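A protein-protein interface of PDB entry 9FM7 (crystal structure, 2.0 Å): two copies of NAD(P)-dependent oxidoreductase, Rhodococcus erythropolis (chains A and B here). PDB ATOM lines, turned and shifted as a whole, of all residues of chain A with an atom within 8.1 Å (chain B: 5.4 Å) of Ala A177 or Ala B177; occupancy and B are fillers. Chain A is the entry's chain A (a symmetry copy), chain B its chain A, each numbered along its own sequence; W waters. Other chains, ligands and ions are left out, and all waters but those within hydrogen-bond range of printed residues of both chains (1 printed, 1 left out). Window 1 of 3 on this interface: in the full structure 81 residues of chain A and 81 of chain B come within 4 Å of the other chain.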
ATOM      1  N   MET A 169      22.155  21.526  23.963  1.00  0.00           N
ATOM      2  CA  MET A 169      21.614  20.381  23.250  1.00  0.00           C
ATOM      3  C   MET A 169      22.606  19.226  23.228  1.00  0.00           C
ATOM      4  O   MET A 169      22.213  18.099  23.469  1.00  0.00           O
ATOM      5  CB  MET A 169      21.220  20.741  21.816  1.00  0.00           C
ATOM      6  CG  MET A 169      20.082  21.706  21.742  1.00  0.00           C
ATOM      7  SD  MET A 169      18.627  21.062  22.574  1.00  0.00           S
ATOM      8  CE  MET A 169      17.406  21.321  21.288  1.00  0.00           C
ATOM      9  N   ALA A 170      23.890  19.492  23.020  1.00  0.00           N
ATOM     10  CA  ALA A 170      24.880  18.432  22.940  1.00  0.00           C
ATOM     11  C   ALA A 170      25.257  17.943  24.328  1.00  0.00           C
ATOM     12  O   ALA A 170      25.597  16.779  24.488  1.00  0.00           O
ATOM     13  CB  ALA A 170      26.127  18.877  22.196  1.00  0.00           C
ATOM     14  N   GLY A 171      25.225  18.854  25.301  1.00  0.00           N
ATOM     15  CA  GLY A 171      25.736  18.568  26.630  1.00  0.00           C
ATOM     16  C   GLY A 171      24.621  18.236  27.600  1.00  0.00           C
ATOM     17  O   GLY A 171      24.415  17.064  27.909  1.00  0.00           O
ATOM     18  N   ALA A 172      23.868  19.269  27.992  1.00  0.00           N
ATOM     19  CA  ALA A 172      22.850  19.166  29.027  1.00  0.00           C
ATOM     20  C   ALA A 172      21.776  18.148  28.675  1.00  0.00           C
ATOM     21  O   ALA A 172      21.274  17.470  29.564  1.00  0.00           O
ATOM     22  CB  ALA A 172      22.226  20.525  29.257  1.00  0.00           C
ATOM     23  N   PHE A 173      21.403  18.096  27.386  1.00  0.00           N
ATOM     24  CA  PHE A 173      20.418  17.144  26.898  1.00  0.00           C
ATOM     25  C   PHE A 173      21.098  15.858  26.423  1.00  0.00           C
ATOM     26  O   PHE A 173      20.989  14.798  27.032  1.00  0.00           O
ATOM     27  CB  PHE A 173      19.527  17.764  25.802  1.00  0.00           C
ATOM     28  CG  PHE A 173      18.683  16.672  25.163  1.00  0.00           C
ATOM     29  CD1 PHE A 173      17.711  16.020  25.912  1.00  0.00           C
ATOM     30  CD2 PHE A 173      18.891  16.258  23.848  1.00  0.00           C
ATOM     31  CE1 PHE A 173      16.979  14.968  25.380  1.00  0.00           C
ATOM     32  CE2 PHE A 173      18.128  15.230  23.302  1.00  0.00           C
ATOM     33  CZ  PHE A 173      17.173  14.582  24.070  1.00  0.00           C
ATOM     34  N   PHE A 174      21.845  15.931  25.322  1.00  0.00           N
ATOM     35  CA  PHE A 174      22.187  14.720  24.595  1.00  0.00           C
ATOM     36  C   PHE A 174      23.118  13.799  25.382  1.00  0.00           C
ATOM     37  O   PHE A 174      22.885  12.597  25.460  1.00  0.00           O
ATOM     38  CB  PHE A 174      22.856  15.120  23.279  1.00  0.00           C
ATOM     39  CG  PHE A 174      23.156  13.939  22.372  1.00  0.00           C
ATOM     40  CD1 PHE A 174      22.225  13.507  21.436  1.00  0.00           C
ATOM     41  CD2 PHE A 174      24.373  13.289  22.437  1.00  0.00           C
ATOM     42  CE1 PHE A 174      22.513  12.450  20.578  1.00  0.00           C
ATOM     43  CE2 PHE A 174      24.643  12.214  21.598  1.00  0.00           C
ATOM     44  CZ  PHE A 174      23.723  11.825  20.643  1.00  0.00           C
ATOM     45  N   ASN A 175      24.212  14.340  25.893  1.00  0.00           N
ATOM     46  CA  ASN A 175      25.226  13.516  26.525  1.00  0.00           C
ATOM     47  C   ASN A 175      24.648  12.840  27.768  1.00  0.00           C
ATOM     48  O   ASN A 175      24.951  11.674  28.055  1.00  0.00           O
ATOM     49  CB  ASN A 175      26.470  14.327  26.844  1.00  0.00           C
ATOM     50  CG  ASN A 175      27.597  13.437  27.296  1.00  0.00           C
ATOM     51  OD1 ASN A 175      28.192  12.719  26.489  1.00  0.00           O
ATOM     52  ND2 ASN A 175      27.899  13.476  28.575  1.00  0.00           N
ATOM     53  N   VAL A 176      23.805  13.585  28.478  1.00  0.00           N
ATOM     54  CA  VAL A 176      23.180  13.118  29.703  1.00  0.00           C
ATOM     55  C   VAL A 176      22.168  12.036  29.380  1.00  0.00           C
ATOM     56  O   VAL A 176      22.105  11.012  30.054  1.00  0.00           O
ATOM     57  CB  VAL A 176      22.508  14.245  30.492  1.00  0.00           C
ATOM     58  CG1 VAL A 176      21.638  13.721  31.610  1.00  0.00           C
ATOM     59  CG2 VAL A 176      23.545  15.235  31.000  1.00  0.00           C
ATOM     60  N   ALA A 177      21.381  12.273  28.339  1.00  0.00           N
ATOM     61  CA  ALA A 177      20.411  11.282  27.918  1.00  0.00           C
ATOM     62  C   ALA A 177      21.125  10.007  27.468  1.00  0.00           C
ATOM     63  O   ALA A 177      20.630   8.911  27.700  1.00  0.00           O
ATOM     64  CB  ALA A 177      19.550  11.882  26.816  1.00  0.00           C
ATOM     65  N   LEU A 178      22.276  10.137  26.805  1.00  0.00           N
ATOM     66  CA  LEU A 178      23.059   8.974  26.441  1.00  0.00           C
ATOM     67  C   LEU A 178      23.544   8.215  27.685  1.00  0.00           C
ATOM     68  O   LEU A 178      23.471   6.975  27.751  1.00  0.00           O
ATOM     69  CB  LEU A 178      24.219   9.391  25.546  1.00  0.00           C
ATOM     70  CG  LEU A 178      25.162   8.259  25.140  1.00  0.00           C
ATOM     71  CD1 LEU A 178      24.431   7.257  24.282  1.00  0.00           C
ATOM     72  CD2 LEU A 178      26.376   8.846  24.439  1.00  0.00           C
ATOM     73  N   GLY A 179      23.992   8.962  28.695  1.00  0.00           N
ATOM     74  CA  GLY A 179      24.339   8.357  29.977  1.00  0.00           C
ATOM     75  C   GLY A 179      23.165   7.607  30.613  1.00  0.00           C
ATOM     76  O   GLY A 179      23.336   6.488  31.125  1.00  0.00           O
ATOM     77  N   ALA A 180      21.971   8.225  30.553  1.00  0.00           N
ATOM     78  CA  ALA A 180      20.781   7.651  31.154  1.00  0.00           C
ATOM     79  C   ALA A 180      20.541   6.263  30.576  1.00  0.00           C
ATOM     80  O   ALA A 180      20.149   5.339  31.287  1.00  0.00           O
ATOM     81  CB  ALA A 180      19.612   8.564  30.925  1.00  0.00           C
ATOM     82  N   PHE A 181      20.757   6.135  29.263  1.00  0.00           N
ATOM     83  CA  PHE A 181      20.601   4.869  28.559  1.00  0.00           C
ATOM     84  C   PHE A 181      21.622   3.839  29.055  1.00  0.00           C
ATOM     85  O   PHE A 181      21.304   2.653  29.092  1.00  0.00           O
ATOM     86  CB  PHE A 181      20.702   5.025  27.035  1.00  0.00           C
ATOM     87  CG  PHE A 181      20.407   3.724  26.283  1.00  0.00           C
ATOM     88  CD1 PHE A 181      19.119   3.220  26.209  1.00  0.00           C
ATOM     89  CD2 PHE A 181      21.421   3.013  25.656  1.00  0.00           C
ATOM     90  CE1 PHE A 181      18.850   2.036  25.538  1.00  0.00           C
ATOM     91  CE2 PHE A 181      21.153   1.811  25.006  1.00  0.00           C
ATOM     92  CZ  PHE A 181      19.874   1.340  24.923  1.00  0.00           C
ATOM     93  N   HIS A 182      22.843   4.257  29.406  1.00  0.00           N
ATOM     94  CA  HIS A 182      23.811   3.341  30.018  1.00  0.00           C
ATOM     95  C   HIS A 182      23.284   2.810  31.366  1.00  0.00           C
ATOM     96  O   HIS A 182      23.338   1.606  31.618  1.00  0.00           O
ATOM     97  CB  HIS A 182      25.184   4.000  30.173  1.00  0.00           C
ATOM     98  CG  HIS A 182      25.936   4.250  28.905  1.00  0.00           C
ATOM     99  ND1 HIS A 182      25.543   5.138  27.924  1.00  0.00           N
ATOM    100  CD2 HIS A 182      27.076   3.710  28.482  1.00  0.00           C
ATOM    101  CE1 HIS A 182      26.438   5.097  26.932  1.00  0.00           C
ATOM    102  NE2 HIS A 182      27.399   4.236  27.276  1.00  0.00           N
ATOM    103  N   GLU A 183      22.756   3.700  32.221  1.00  0.00           N
ATOM    104  CA  GLU A 183      22.121   3.280  33.458  1.00  0.00           C
ATOM    105  C   GLU A 183      20.974   2.305  33.147  1.00  0.00           C
ATOM    106  O   GLU A 183      20.771   1.322  33.863  1.00  0.00           O
ATOM    107  CB  GLU A 183      21.645   4.458  34.312  1.00  0.00           C
ATOM    108  CG  GLU A 183      22.744   5.383  34.842  1.00  0.00           C
ATOM    109  CD  GLU A 183      22.352   6.352  35.968  1.00  0.00           C
ATOM    110  OE1 GLU A 183      21.141   6.347  36.356  1.00  0.00           O
ATOM    111  OE2 GLU A 183      23.237   7.148  36.440  1.00  0.00           O
ATOM    112  N   ALA A 184      20.193   2.572  32.096  1.00  0.00           N
ATOM    113  CA  ALA A 184      19.041   1.733  31.816  1.00  0.00           C
ATOM    114  C   ALA A 184      19.520   0.317  31.502  1.00  0.00           C
ATOM    115  O   ALA A 184      19.055  -0.642  32.109  1.00  0.00           O
ATOM    116  CB  ALA A 184      18.204   2.315  30.687  1.00  0.00           C
ATOM    117  N   TRP A 205      10.735   4.833  21.534  1.00  0.00           N
ATOM    118  CA  TRP A 205      11.021   5.691  22.683  1.00  0.00           C
ATOM    119  C   TRP A 205      11.626   7.043  22.260  1.00  0.00           C
ATOM    120  O   TRP A 205      11.288   8.076  22.833  1.00  0.00           O
ATOM    121  CB  TRP A 205      11.911   4.912  23.659  1.00  0.00           C
ATOM    122  CG  TRP A 205      11.154   3.858  24.439  1.00  0.00           C
ATOM    123  CD1 TRP A 205      11.234   2.506  24.300  1.00  0.00           C
ATOM    124  CD2 TRP A 205      10.179   4.083  25.473  1.00  0.00           C
ATOM    125  NE1 TRP A 205      10.377   1.875  25.166  1.00  0.00           N
ATOM    126  CE2 TRP A 205       9.722   2.818  25.900  1.00  0.00           C
ATOM    127  CE3 TRP A 205       9.665   5.225  26.092  1.00  0.00           C
ATOM    128  CZ2 TRP A 205       8.801   2.666  26.924  1.00  0.00           C
ATOM    129  CZ3 TRP A 205       8.755   5.073  27.110  1.00  0.00           C
ATOM    130  CH2 TRP A 205       8.341   3.811  27.523  1.00  0.00           C
ATOM    131  N   LEU A 209       9.951  10.658  22.706  1.00  0.00           N
ATOM    132  CA  LEU A 209      10.728  11.681  23.414  1.00  0.00           C
ATOM    133  C   LEU A 209      10.674  12.987  22.629  1.00  0.00           C
ATOM    134  O   LEU A 209      10.481  14.071  23.200  1.00  0.00           O
ATOM    135  CB  LEU A 209      12.173  11.227  23.601  1.00  0.00           C
ATOM    136  CG  LEU A 209      13.111  12.190  24.351  1.00  0.00           C
ATOM    137  CD1 LEU A 209      12.559  12.468  25.741  1.00  0.00           C
ATOM    138  CD2 LEU A 209      14.521  11.668  24.460  1.00  0.00           C
ATOM    139  N   LEU A 213       9.481  16.560  23.957  1.00  0.00           N
ATOM    140  CA  LEU A 213      10.359  17.724  23.956  1.00  0.00           C
ATOM    141  C   LEU A 213       9.632  18.933  23.358  1.00  0.00           C
ATOM    142  O   LEU A 213       9.751  20.054  23.850  1.00  0.00           O
ATOM    143  CB  LEU A 213      11.653  17.475  23.180  1.00  0.00           C
ATOM    144  CG  LEU A 213      12.549  16.329  23.655  1.00  0.00           C
ATOM    145  CD1 LEU A 213      13.886  16.381  22.981  1.00  0.00           C
ATOM    146  CD2 LEU A 213      12.685  16.315  25.158  1.00  0.00           C
ATOM    147  N   LEU A 255      22.154   9.154  37.935  1.00  0.00           N
ATOM    148  CA  LEU A 255      21.280  10.046  37.165  1.00  0.00           C
ATOM    149  C   LEU A 255      19.846   9.940  37.678  1.00  0.00           C
ATOM    150  O   LEU A 255      19.118  10.943  37.784  1.00  0.00           O
ATOM    151  CB  LEU A 255      21.354   9.726  35.672  1.00  0.00           C
ATOM    152  CG  LEU A 255      22.689  10.014  34.985  1.00  0.00           C
ATOM    153  CD1 LEU A 255      22.872   9.334  33.629  1.00  0.00           C
ATOM    154  CD2 LEU A 255      22.813  11.535  34.856  1.00  0.00           C
ATOM    155  N   ASN A 259      17.626  13.068  39.116  1.00  0.00           N
ATOM    156  CA  ASN A 259      16.298  13.318  38.571  1.00  0.00           C
ATOM    157  C   ASN A 259      15.257  13.417  39.693  1.00  0.00           C
ATOM    158  O   ASN A 259      14.439  14.329  39.703  1.00  0.00           O
ATOM    159  CB  ASN A 259      15.984  12.195  37.581  1.00  0.00           C
ATOM    160  CG  ASN A 259      14.645  12.317  36.895  1.00  0.00           C
ATOM    161  OD1 ASN A 259      14.211  13.404  36.494  1.00  0.00           O
ATOM    162  ND2 ASN A 259      13.984  11.173  36.733  1.00  0.00           N
ATOM    163  N   GLN A 279       8.739  21.329  36.533  1.00  0.00           N
ATOM    164  CA  GLN A 279       9.999  21.063  37.203  1.00  0.00           C
ATOM    165  C   GLN A 279      11.079  22.066  36.778  1.00  0.00           C
ATOM    166  O   GLN A 279      12.088  22.240  37.470  1.00  0.00           O
ATOM    167  CB  GLN A 279      10.493  19.628  37.042  1.00  0.00           C
ATOM    168  CG  GLN A 279      11.178  19.326  35.713  1.00  0.00           C
ATOM    169  CD  GLN A 279      11.766  17.936  35.647  1.00  0.00           C
ATOM    170  OE1 GLN A 279      11.265  17.064  34.926  1.00  0.00           O
ATOM    171  NE2 GLN A 279      12.817  17.707  36.425  1.00  0.00           N
ATOM    172  N   ALA B 172      14.657   4.858  33.703  1.00  0.00           N
ATOM    173  CA  ALA B 172      16.092   5.107  33.705  1.00  0.00           C
ATOM    174  C   ALA B 172      16.537   5.905  32.490  1.00  0.00           C
ATOM    175  O   ALA B 172      17.442   6.725  32.606  1.00  0.00           O
ATOM    176  CB  ALA B 172      16.832   3.788  33.764  1.00  0.00           C
ATOM    177  N   PHE B 173      15.928   5.614  31.329  1.00  0.00           N
ATOM    178  CA  PHE B 173      16.223   6.325  30.095  1.00  0.00           C
ATOM    179  C   PHE B 173      15.283   7.521  29.922  1.00  0.00           C
ATOM    180  O   PHE B 173      15.674   8.679  30.019  1.00  0.00           O
ATOM    181  CB  PHE B 173      16.186   5.381  28.876  1.00  0.00           C
ATOM    182  CG  PHE B 173      16.262   6.204  27.600  1.00  0.00           C
ATOM    183  CD1 PHE B 173      17.416   6.921  27.305  1.00  0.00           C
ATOM    184  CD2 PHE B 173      15.178   6.312  26.730  1.00  0.00           C
ATOM    185  CE1 PHE B 173      17.488   7.741  26.188  1.00  0.00           C
ATOM    186  CE2 PHE B 173      15.265   7.104  25.588  1.00  0.00           C
ATOM    187  CZ  PHE B 173      16.420   7.822  25.319  1.00  0.00           C
ATOM    188  N   PHE B 174      13.999   7.259  29.682  1.00  0.00           N
ATOM    189  CA  PHE B 174      13.141   8.290  29.121  1.00  0.00           C
ATOM    190  C   PHE B 174      12.910   9.456  30.082  1.00  0.00           C
ATOM    191  O   PHE B 174      13.018  10.615  29.693  1.00  0.00           O
ATOM    192  CB  PHE B 174      11.798   7.654  28.757  1.00  0.00           C
ATOM    193  CG  PHE B 174      10.852   8.609  28.051  1.00  0.00           C
ATOM    194  CD1 PHE B 174      10.852   8.716  26.666  1.00  0.00           C
ATOM    195  CD2 PHE B 174       9.948   9.369  28.769  1.00  0.00           C
ATOM    196  CE1 PHE B 174       9.959   9.562  26.015  1.00  0.00           C
ATOM    197  CE2 PHE B 174       9.079  10.235  28.113  1.00  0.00           C
ATOM    198  CZ  PHE B 174       9.063  10.296  26.734  1.00  0.00           C
ATOM    199  N   ASN B 175      12.513   9.158  31.309  1.00  0.00           N
ATOM    200  CA  ASN B 175      12.126  10.202  32.241  1.00  0.00           C
ATOM    201  C   ASN B 175      13.326  11.095  32.551  1.00  0.00           C
ATOM    202  O   ASN B 175      13.189  12.320  32.679  1.00  0.00           O
ATOM    203  CB  ASN B 175      11.514   9.612  33.499  1.00  0.00           C
ATOM    204  CG  ASN B 175      10.917  10.686  34.368  1.00  0.00           C
ATOM    205  OD1 ASN B 175       9.866  11.246  34.041  1.00  0.00           O
ATOM    206  ND2 ASN B 175      11.568  10.982  35.470  1.00  0.00           N
ATOM    207  N   VAL B 176      14.493  10.463  32.648  1.00  0.00           N
ATOM    208  CA  VAL B 176      15.735  11.146  32.963  1.00  0.00           C
ATOM    209  C   VAL B 176      16.150  12.018  31.796  1.00  0.00           C
ATOM    210  O   VAL B 176      16.555  13.163  31.977  1.00  0.00           O
ATOM    211  CB  VAL B 176      16.867  10.179  33.322  1.00  0.00           C
ATOM    212  CG1 VAL B 176      18.210  10.869  33.384  1.00  0.00           C
ATOM    213  CG2 VAL B 176      16.552   9.442  34.615  1.00  0.00           C
ATOM    214  N   ALA B 177      16.037  11.467  30.593  1.00  0.00           N
ATOM    215  CA  ALA B 177      16.362  12.234  29.407  1.00  0.00           C
ATOM    216  C   ALA B 177      15.417  13.428  29.276  1.00  0.00           C
ATOM    217  O   ALA B 177      15.831  14.494  28.842  1.00  0.00           O
ATOM    218  CB  ALA B 177      16.298  11.310  28.199  1.00  0.00           C
ATOM    219  N   LEU B 178      14.141  13.253  29.629  1.00  0.00           N
ATOM    220  CA  LEU B 178      13.213  14.366  29.632  1.00  0.00           C
ATOM    221  C   LEU B 178      13.633  15.440  30.646  1.00  0.00           C
ATOM    222  O   LEU B 178      13.613  16.649  30.347  1.00  0.00           O
ATOM    223  CB  LEU B 178      11.801  13.861  29.898  1.00  0.00           C
ATOM    224  CG  LEU B 178      10.731  14.949  29.988  1.00  0.00           C
ATOM    225  CD1 LEU B 178      10.585  15.644  28.657  1.00  0.00           C
ATOM    226  CD2 LEU B 178       9.427  14.330  30.465  1.00  0.00           C
ATOM    227  N   GLY B 179      14.064  15.002  31.829  1.00  0.00           N
ATOM    228  CA  GLY B 179      14.625  15.923  32.811  1.00  0.00           C
ATOM    229  C   GLY B 179      15.840  16.689  32.278  1.00  0.00           C
ATOM    230  O   GLY B 179      15.956  17.908  32.483  1.00  0.00           O
ATOM    231  N   ALA B 180      16.726  15.963  31.572  1.00  0.00           N
ATOM    232  CA  ALA B 180      17.946  16.547  31.044  1.00  0.00           C
ATOM    233  C   ALA B 180      17.596  17.730  30.150  1.00  0.00           C
ATOM    234  O   ALA B 180      18.276  18.754  30.158  1.00  0.00           O
ATOM    235  CB  ALA B 180      18.728  15.499  30.307  1.00  0.00           C
ATOM    236  N   PHE B 181      16.535  17.562  29.355  1.00  0.00           N
ATOM    237  CA  PHE B 181      16.050  18.603  28.459  1.00  0.00           C
ATOM    238  C   PHE B 181      15.546  19.815  29.253  1.00  0.00           C
ATOM    239  O   PHE B 181      15.690  20.939  28.781  1.00  0.00           O
ATOM    240  CB  PHE B 181      14.956  18.100  27.507  1.00  0.00           C
ATOM    241  CG  PHE B 181      14.536  19.152  26.476  1.00  0.00           C
ATOM    242  CD1 PHE B 181      15.376  19.499  25.429  1.00  0.00           C
ATOM    243  CD2 PHE B 181      13.305  19.787  26.559  1.00  0.00           C
ATOM    244  CE1 PHE B 181      15.003  20.458  24.499  1.00  0.00           C
ATOM    245  CE2 PHE B 181      12.944  20.769  25.640  1.00  0.00           C
ATOM    246  CZ  PHE B 181      13.773  21.082  24.603  1.00  0.00           C
ATOM    247  N   LEU B 209      20.376  10.604  18.535  1.00  0.00           N
ATOM    248  CA  LEU B 209      20.388   9.857  19.797  1.00  0.00           C
ATOM    249  C   LEU B 209      20.019   8.403  19.525  1.00  0.00           C
ATOM    250  O   LEU B 209      20.651   7.473  20.048  1.00  0.00           O
ATOM    251  CB  LEU B 209      19.421  10.478  20.801  1.00  0.00           C
ATOM    252  CG  LEU B 209      19.340   9.814  22.187  1.00  0.00           C
ATOM    253  CD1 LEU B 209      20.711   9.823  22.843  1.00  0.00           C
ATOM    254  CD2 LEU B 209      18.337  10.479  23.097  1.00  0.00           C
ATOM    255  N   LEU B 213      22.129   5.151  20.486  1.00  0.00           N
ATOM    256  CA  LEU B 213      21.600   4.109  21.358  1.00  0.00           C
ATOM    257  C   LEU B 213      21.838   2.729  20.736  1.00  0.00           C
ATOM    258  O   LEU B 213      22.193   1.773  21.424  1.00  0.00           O
ATOM    259  CB  LEU B 213      20.108   4.288  21.638  1.00  0.00           C
ATOM    260  CG  LEU B 213      19.669   5.595  22.304  1.00  0.00           C
ATOM    261  CD1 LEU B 213      18.243   5.511  22.757  1.00  0.00           C
ATOM    262  CD2 LEU B 213      20.590   5.977  23.437  1.00  0.00           C
HETATM  263  O   HOH W   1      18.673   6.506  35.201  1.00  0.00           O
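Of the 12 printed residues of chain B, 10 touch a printed residue of chain A.
Printed residues of chain B that touch a printed residue of chain A: Ala B172, Phe B173, Phe B174, Asn B175, Val B176, Ala B177, Ala B180, Phe B181, Leu B209 and Leu B213.
Hydrophobic or aromatic side chains of chain B that line the printed part of chain A: Ala B172, Phe B173, Phe B174, Val B176, Ala B177, Ala B180, Phe B181, Leu B209 and Leu B213.
Of the 22 printed residues of chain A, 12 touch a printed residue of chain B.
Among the printed residues, no Asp or Glu carboxylate lies within 4 Å of a Lys or Arg side-chain nitrogen of the other chain.
Among the printed residues, merely in contact across the chains: Leu A209 with Phe B174 (3.4 Å), Phe A174 with Leu B209 (3.4 Å), Ala A177 with Ala B177 (3.6 Å), Ala A184 with Ala B172 (3.6 Å), Phe A181 with Leu B213 (3.6 Å), Leu A213 with Phe B181 (3.6 Å), Ala A180 with Val B176 (3.7 Å), Val A176 with Ala B180 (3.7 Å), Ala A177 with Phe B173 (3.7 Å), Phe A173 with Ala B177 (3.7 Å), Trp A205 with Phe B174 (3.7 Å), Asn A259 with Val B176 (3.8 Å), Phe A173 with Phe B181 (3.8 Å) and Phe A181 with Phe B173 (3.8 Å).
Of chain B, only Phe B173 (3.7 Å) and Ala B177 (3.6 Å) come within 4 Å of Ala A177.
Of chain A, only Phe A173 (3.7 Å) and Ala A177 (3.6 Å) come within 4 Å of Ala B177.
Printed residues of chain A within 4 Å of Leu B213: Phe A181.
Of the printed residues of chain B, Asn A259 touches Asn B175 (2.7 Å) and Val B176 (3.8 Å).
Of the printed residues of chain A, Phe B173 touches Ala A177 (3.7 Å) and Phe A181 (3.8 Å).
Met A169 touches none of the printed residues of chain B.
Asn A175 touches none of the printed residues of chain B.
The nearest residue of chain B that does not touch Ala A177 is Leu B209 (4.2 Å).
The nearest residue of chain A that does not touch Ala B177 is Leu A209 (4.2 Å).
Ala A172 touches Ala B180, and with the chains exchanged Ala A180 touches Ala B172.
Phe A173 touches Ala B177, and with the chains exchanged Ala A177 touches Phe B173.
Val A176 touches Ala B180, and with the chains exchanged Ala A180 touches Val B176.
Ala A177 touches its own counterpart, Ala B177.
12 positions are printed for both chains.
Water W1 bridges OE1 of Glu A183 (2.7 Å) and O of Ala B172 (2.9 Å).
The backbone carbonyl oxygen of Met A169 lies within hydrogen-bond range of the backbone NH of Phe A174, at 2.9 Å.
ND2 of Asn A259 lies close to ND2 of Asn B175 (2.7 Å).
The backbone carbonyl oxygen of Ala B180 lies close to the backbone carbonyl oxygen of Ala A172 (3.3 Å).
O of Ala A180 sits close to O of Ala B172.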
